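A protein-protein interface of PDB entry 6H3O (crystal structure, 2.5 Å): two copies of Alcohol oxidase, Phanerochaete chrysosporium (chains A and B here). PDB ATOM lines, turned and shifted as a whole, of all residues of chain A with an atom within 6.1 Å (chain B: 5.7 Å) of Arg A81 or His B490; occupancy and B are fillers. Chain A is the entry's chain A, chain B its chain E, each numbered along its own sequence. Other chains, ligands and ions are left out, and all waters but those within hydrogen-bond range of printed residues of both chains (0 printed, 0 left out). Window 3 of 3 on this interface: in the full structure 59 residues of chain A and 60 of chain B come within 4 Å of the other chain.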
ATOM      1  N   SER A  77      13.261 -11.625  24.083  1.00  0.00           N
ATOM      2  CA  SER A  77      13.188 -10.599  23.044  1.00  0.00           C
ATOM      3  C   SER A  77      11.754 -10.067  22.920  1.00  0.00           C
ATOM      4  O   SER A  77      10.836 -10.810  22.582  1.00  0.00           O
ATOM      5  CB  SER A  77      13.684 -11.144  21.724  1.00  0.00           C
ATOM      6  OG  SER A  77      13.093 -10.462  20.628  1.00  0.00           O
ATOM      7  N   SER A  78      11.594  -8.764  23.179  1.00  0.00           N
ATOM      8  CA  SER A  78      10.333  -8.019  23.025  1.00  0.00           C
ATOM      9  C   SER A  78       9.765  -8.214  21.615  1.00  0.00           C
ATOM     10  O   SER A  78       8.552  -8.378  21.448  1.00  0.00           O
ATOM     11  CB  SER A  78      10.550  -6.549  23.303  1.00  0.00           C
ATOM     12  OG  SER A  78      11.563  -6.013  22.449  1.00  0.00           O
ATOM     13  N   TYR A  79      10.669  -8.207  20.625  1.00  0.00           N
ATOM     14  CA  TYR A  79      10.338  -8.190  19.190  1.00  0.00           C
ATOM     15  C   TYR A  79       9.719  -9.523  18.739  1.00  0.00           C
ATOM     16  O   TYR A  79       9.118  -9.581  17.668  1.00  0.00           O
ATOM     17  CB  TYR A  79      11.580  -7.846  18.360  1.00  0.00           C
ATOM     18  CG  TYR A  79      12.254  -6.553  18.752  1.00  0.00           C
ATOM     19  CD1 TYR A  79      11.814  -5.330  18.264  1.00  0.00           C
ATOM     20  CD2 TYR A  79      13.317  -6.547  19.639  1.00  0.00           C
ATOM     21  CE1 TYR A  79      12.418  -4.138  18.632  1.00  0.00           C
ATOM     22  CE2 TYR A  79      13.932  -5.365  20.019  1.00  0.00           C
ATOM     23  CZ  TYR A  79      13.483  -4.155  19.515  1.00  0.00           C
ATOM     24  OH  TYR A  79      14.104  -2.997  19.892  1.00  0.00           O
ATOM     25  N   LEU A  80       9.861 -10.580  19.553  1.00  0.00           N
ATOM     26  CA  LEU A  80       9.299 -11.905  19.262  1.00  0.00           C
ATOM     27  C   LEU A  80       8.251 -12.282  20.321  1.00  0.00           C
ATOM     28  O   LEU A  80       8.016 -13.476  20.563  1.00  0.00           O
ATOM     29  CB  LEU A  80      10.442 -12.929  19.221  1.00  0.00           C
ATOM     30  CG  LEU A  80      11.597 -12.608  18.268  1.00  0.00           C
ATOM     31  CD1 LEU A  80      12.705 -13.648  18.375  1.00  0.00           C
ATOM     32  CD2 LEU A  80      11.108 -12.504  16.832  1.00  0.00           C
ATOM     33  N   ARG A  81       7.627 -11.258  20.927  1.00  0.00           N
ATOM     34  CA  ARG A  81       6.574 -11.371  21.966  1.00  0.00           C
ATOM     35  C   ARG A  81       7.040 -12.232  23.152  1.00  0.00           C
ATOM     36  O   ARG A  81       6.227 -12.963  23.758  1.00  0.00           O
ATOM     37  CB  ARG A  81       5.286 -11.958  21.379  1.00  0.00           C
ATOM     38  CG  ARG A  81       4.879 -11.382  20.033  1.00  0.00           C
ATOM     39  CD  ARG A  81       3.635 -12.093  19.543  1.00  0.00           C
ATOM     40  NE  ARG A  81       2.399 -11.476  19.993  1.00  0.00           N
ATOM     41  CZ  ARG A  81       1.218 -12.080  20.001  1.00  0.00           C
ATOM     42  NH1 ARG A  81       1.133 -13.380  19.770  1.00  0.00           N
ATOM     43  NH2 ARG A  81       0.126 -11.375  20.236  1.00  0.00           N
ATOM     44  N   GLY A  82       8.338 -12.150  23.479  1.00  0.00           N
ATOM     45  CA  GLY A  82       8.899 -12.749  24.691  1.00  0.00           C
ATOM     46  C   GLY A  82       9.606 -14.086  24.486  1.00  0.00           C
ATOM     47  O   GLY A  82      10.023 -14.692  25.475  1.00  0.00           O
ATOM     48  N   ARG A  83       9.772 -14.550  23.236  1.00  0.00           N
ATOM     49  CA  ARG A  83      10.583 -15.761  22.959  1.00  0.00           C
ATOM     50  C   ARG A  83      12.055 -15.490  23.303  1.00  0.00           C
ATOM     51  O   ARG A  83      12.507 -14.333  23.341  1.00  0.00           O
ATOM     52  CB  ARG A  83      10.516 -16.215  21.492  1.00  0.00           C
ATOM     53  CG  ARG A  83       9.121 -16.558  20.979  1.00  0.00           C
ATOM     54  CD  ARG A  83       9.029 -17.344  19.671  1.00  0.00           C
ATOM     55  NE  ARG A  83      10.290 -17.686  19.005  1.00  0.00           N
ATOM     56  CZ  ARG A  83      10.618 -17.399  17.740  1.00  0.00           C
ATOM     57  NH1 ARG A  83       9.867 -16.594  17.007  1.00  0.00           N
ATOM     58  NH2 ARG A  83      11.710 -17.927  17.214  1.00  0.00           N
ATOM     59  N   ARG A 488      -3.365 -16.411  13.923  1.00  0.00           N
ATOM     60  CA  ARG A 488      -4.532 -16.424  14.763  1.00  0.00           C
ATOM     61  C   ARG A 488      -5.623 -15.521  14.170  1.00  0.00           C
ATOM     62  O   ARG A 488      -6.060 -14.562  14.822  1.00  0.00           O
ATOM     63  CB  ARG A 488      -4.117 -15.969  16.165  1.00  0.00           C
ATOM     64  CG  ARG A 488      -2.994 -16.806  16.761  1.00  0.00           C
ATOM     65  CD  ARG A 488      -2.779 -16.565  18.241  1.00  0.00           C
ATOM     66  NE  ARG A 488      -2.337 -17.772  18.928  1.00  0.00           N
ATOM     67  CZ  ARG A 488      -2.080 -17.837  20.223  1.00  0.00           C
ATOM     68  NH1 ARG A 488      -2.085 -16.728  20.943  1.00  0.00           N
ATOM     69  NH2 ARG A 488      -1.844 -19.005  20.796  1.00  0.00           N
ATOM     70  N   LYS A 546      -2.399  -8.091  10.923  1.00  0.00           N
ATOM     71  CA  LYS A 546      -1.871  -8.001  12.287  1.00  0.00           C
ATOM     72  C   LYS A 546      -1.575  -9.404  12.854  1.00  0.00           C
ATOM     73  O   LYS A 546      -0.601  -9.581  13.599  1.00  0.00           O
ATOM     74  CB  LYS A 546      -2.860  -7.217  13.157  1.00  0.00           C
ATOM     75  CG  LYS A 546      -2.271  -6.608  14.416  1.00  0.00           C
ATOM     76  CD  LYS A 546      -2.384  -7.515  15.611  1.00  0.00           C
ATOM     77  CE  LYS A 546      -1.504  -7.071  16.759  1.00  0.00           C
ATOM     78  NZ  LYS A 546      -2.167  -7.305  18.063  1.00  0.00           N
ATOM     79  N   ASP A 550       1.978 -11.199  13.974  1.00  0.00           N
ATOM     80  CA  ASP A 550       2.138 -11.817  15.296  1.00  0.00           C
ATOM     81  C   ASP A 550       2.682 -13.248  15.153  1.00  0.00           C
ATOM     82  O   ASP A 550       3.536 -13.671  15.937  1.00  0.00           O
ATOM     83  CB  ASP A 550       0.820 -11.778  16.074  1.00  0.00           C
ATOM     84  CG  ASP A 550       0.439 -10.397  16.591  1.00  0.00           C
ATOM     85  OD1 ASP A 550       1.344  -9.555  16.779  1.00  0.00           O
ATOM     86  OD2 ASP A 550      -0.767 -10.171  16.793  1.00  0.00           O
ATOM     87  N   TRP A 551       2.167 -13.967  14.148  1.00  0.00           N
ATOM     88  CA  TRP A 551       2.605 -15.309  13.749  1.00  0.00           C
ATOM     89  C   TRP A 551       4.088 -15.305  13.348  1.00  0.00           C
ATOM     90  O   TRP A 551       4.819 -16.248  13.654  1.00  0.00           O
ATOM     91  CB  TRP A 551       1.712 -15.799  12.602  1.00  0.00           C
ATOM     92  CG  TRP A 551       2.001 -17.166  12.056  1.00  0.00           C
ATOM     93  CD1 TRP A 551       1.490 -18.352  12.499  1.00  0.00           C
ATOM     94  CD2 TRP A 551       2.797 -17.484  10.900  1.00  0.00           C
ATOM     95  NE1 TRP A 551       1.937 -19.388  11.723  1.00  0.00           N
ATOM     96  CE2 TRP A 551       2.744 -18.889  10.734  1.00  0.00           C
ATOM     97  CE3 TRP A 551       3.567 -16.729  10.009  1.00  0.00           C
ATOM     98  CZ2 TRP A 551       3.429 -19.547   9.714  1.00  0.00           C
ATOM     99  CZ3 TRP A 551       4.242 -17.382   9.001  1.00  0.00           C
ATOM    100  CH2 TRP A 551       4.169 -18.770   8.856  1.00  0.00           C
ATOM    101  N   ALA A 553       6.409 -12.994  14.436  1.00  0.00           N
ATOM    102  CA  ALA A 553       7.042 -12.811  15.751  1.00  0.00           C
ATOM    103  C   ALA A 553       7.070 -14.133  16.534  1.00  0.00           C
ATOM    104  O   ALA A 553       8.093 -14.470  17.144  1.00  0.00           O
ATOM    105  CB  ALA A 553       6.322 -11.741  16.529  1.00  0.00           C
ATOM    106  N   ASP A 554       5.951 -14.872  16.501  1.00  0.00           N
ATOM    107  CA  ASP A 554       5.760 -16.108  17.281  1.00  0.00           C
ATOM    108  C   ASP A 554       6.571 -17.280  16.709  1.00  0.00           C
ATOM    109  O   ASP A 554       6.975 -18.156  17.469  1.00  0.00           O
ATOM    110  CB  ASP A 554       4.282 -16.513  17.350  1.00  0.00           C
ATOM    111  CG  ASP A 554       3.445 -15.697  18.323  1.00  0.00           C
ATOM    112  OD1 ASP A 554       4.041 -15.101  19.248  1.00  0.00           O
ATOM    113  OD2 ASP A 554       2.199 -15.661  18.148  1.00  0.00           O
ATOM    114  N   ARG B 488      -6.241 -18.636  23.052  1.00  0.00           N
ATOM    115  CA  ARG B 488      -5.181 -17.876  22.400  1.00  0.00           C
ATOM    116  C   ARG B 488      -4.600 -16.851  23.382  1.00  0.00           C
ATOM    117  O   ARG B 488      -4.790 -15.640  23.221  1.00  0.00           O
ATOM    118  CB  ARG B 488      -5.742 -17.177  21.156  1.00  0.00           C
ATOM    119  CG  ARG B 488      -6.153 -18.132  20.044  1.00  0.00           C
ATOM    120  CD  ARG B 488      -6.973 -17.497  18.928  1.00  0.00           C
ATOM    121  NE  ARG B 488      -6.847 -18.246  17.680  1.00  0.00           N
ATOM    122  CZ  ARG B 488      -7.353 -17.884  16.505  1.00  0.00           C
ATOM    123  NH1 ARG B 488      -7.986 -16.731  16.366  1.00  0.00           N
ATOM    124  NH2 ARG B 488      -7.227 -18.694  15.469  1.00  0.00           N
ATOM    125  N   PHE B 489      -3.896 -17.343  24.403  1.00  0.00           N
ATOM    126  CA  PHE B 489      -3.161 -16.479  25.317  1.00  0.00           C
ATOM    127  C   PHE B 489      -1.991 -15.848  24.554  1.00  0.00           C
ATOM    128  O   PHE B 489      -1.564 -16.367  23.517  1.00  0.00           O
ATOM    129  CB  PHE B 489      -2.645 -17.268  26.524  1.00  0.00           C
ATOM    130  CG  PHE B 489      -3.703 -18.007  27.306  1.00  0.00           C
ATOM    131  CD1 PHE B 489      -4.766 -17.328  27.880  1.00  0.00           C
ATOM    132  CD2 PHE B 489      -3.633 -19.380  27.480  1.00  0.00           C
ATOM    133  CE1 PHE B 489      -5.741 -18.006  28.594  1.00  0.00           C
ATOM    134  CE2 PHE B 489      -4.608 -20.055  28.196  1.00  0.00           C
ATOM    135  CZ  PHE B 489      -5.658 -19.366  28.754  1.00  0.00           C
ATOM    136  N   HIS B 490      -1.484 -14.725  25.069  1.00  0.00           N
ATOM    137  CA  HIS B 490      -0.225 -14.162  24.611  1.00  0.00           C
ATOM    138  C   HIS B 490       0.896 -15.118  25.023  1.00  0.00           C
ATOM    139  O   HIS B 490       0.878 -15.645  26.131  1.00  0.00           O
ATOM    140  CB  HIS B 490      -0.052 -12.741  25.164  1.00  0.00           C
ATOM    141  CG  HIS B 490       1.077 -11.988  24.542  1.00  0.00           C
ATOM    142  ND1 HIS B 490       2.391 -12.181  24.925  1.00  0.00           N
ATOM    143  CD2 HIS B 490       1.098 -11.062  23.559  1.00  0.00           C
ATOM    144  CE1 HIS B 490       3.172 -11.391  24.220  1.00  0.00           C
ATOM    145  NE2 HIS B 490       2.406 -10.700  23.369  1.00  0.00           N
ATOM    146  N   PRO B 491       1.875 -15.429  24.148  1.00  0.00           N
ATOM    147  CA  PRO B 491       2.965 -16.345  24.503  1.00  0.00           C
ATOM    148  C   PRO B 491       3.777 -16.042  25.776  1.00  0.00           C
ATOM    149  O   PRO B 491       4.386 -16.948  26.317  1.00  0.00           O
ATOM    150  CB  PRO B 491       3.919 -16.233  23.304  1.00  0.00           C
ATOM    151  CG  PRO B 491       3.017 -15.863  22.147  1.00  0.00           C
ATOM    152  CD  PRO B 491       1.944 -14.982  22.749  1.00  0.00           C
ATOM    153  N   ALA B 492       3.804 -14.779  26.220  1.00  0.00           N
ATOM    154  CA  ALA B 492       4.551 -14.374  27.419  1.00  0.00           C
ATOM    155  C   ALA B 492       3.600 -14.072  28.587  1.00  0.00           C
ATOM    156  O   ALA B 492       3.990 -13.422  29.564  1.00  0.00           O
ATOM    157  CB  ALA B 492       5.426 -13.183  27.105  1.00  0.00           C
ATOM    158  N   SER B 493       2.348 -14.528  28.487  1.00  0.00           N
ATOM    159  CA  SER B 493       1.477 -14.568  29.654  1.00  0.00           C
ATOM    160  C   SER B 493       1.928 -15.730  30.537  1.00  0.00           C
ATOM    161  O   SER B 493       2.340 -16.768  30.025  1.00  0.00           O
ATOM    162  CB  SER B 493       0.016 -14.684  29.274  1.00  0.00           C
ATOM    163  OG  SER B 493      -0.778 -15.004  30.412  1.00  0.00           O
ATOM    164  N   ALA B 496      -0.042 -18.870  29.372  1.00  0.00           N
ATOM    165  CA  ALA B 496       0.201 -19.571  28.130  1.00  0.00           C
ATOM    166  C   ALA B 496       0.299 -21.076  28.413  1.00  0.00           C
ATOM    167  O   ALA B 496       0.720 -21.499  29.499  1.00  0.00           O
ATOM    168  CB  ALA B 496       1.449 -19.039  27.475  1.00  0.00           C
ATOM    169  N   ASP B 544      -5.970 -12.296  29.565  1.00  0.00           N
ATOM    170  CA  ASP B 544      -6.115 -13.744  29.563  1.00  0.00           C
ATOM    171  C   ASP B 544      -7.604 -14.136  29.643  1.00  0.00           C
ATOM    172  O   ASP B 544      -8.027 -15.102  28.984  1.00  0.00           O
ATOM    173  CB  ASP B 544      -5.300 -14.352  30.704  1.00  0.00           C
ATOM    174  CG  ASP B 544      -3.800 -14.203  30.517  1.00  0.00           C
ATOM    175  OD1 ASP B 544      -3.329 -14.450  29.397  1.00  0.00           O
ATOM    176  OD2 ASP B 544      -3.114 -13.846  31.488  1.00  0.00           O
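Among the printed residues, merely in contact across the chains: Arg A81 with Pro B491 (3.5 Å), Arg A81 with Ala B492 (3.4 Å) and Asp A554 with Pro B491 (3.2 Å).
NH1 of Arg B488 is in hydrogen-bond range of O of Arg A488.
NH1 of Arg A488 lies within hydrogen-bond range of O of Phe B489, at 2.7 Å.
The guanidinium group (NE) of Arg A81 lies within hydrogen-bond range of a ring nitrogen (NE2) of His B490, at 3.5 Å.
Printed residues of chain A that touch a printed residue of chain B: Arg A81, Arg A488 and Asp A554.
Along chain A the printed residues that touch a printed residue of chain B span positions 81 to 554.
Among the printed residues, no Asp or Glu carboxylate lies within 4 Å of a Lys or Arg side-chain nitrogen of the other chain.
Of the printed residues of chain B, Arg A81 touches His B490, Pro B491 and Ala B492.
Printed residues of chain B within 4 Å of Arg A488: Arg B488 (3.3 Å) and Phe B489 (2.7 Å).
Of the printed residues of chain B, Asp A554 touches Pro B491 (3.2 Å).
Of the printed residues of chain A, Pro B491 touches Arg A81 and Asp A554.
The nearest residue of chain B that does not touch Arg A81 is Phe B489 (5.5 Å).
NH2 of Arg A81 lies within salt-bridge range of OD2 of Asp A550, at 3.8 Å.
NH1 of Arg A81 is in salt-bridge range of OD2 of Asp A554 (3.0 Å).
ND1 of His B490 lies close to N of Ala B492 (3.2 Å).
NH1 of Arg A83 sits close to O of Asp A554 (3.3 Å).
Arg B488 touches its own counterpart, Arg A488.
Of the 6 pairs that touch across the chains among the printed residues, 1 has its exchanged pair printed and touching as well.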
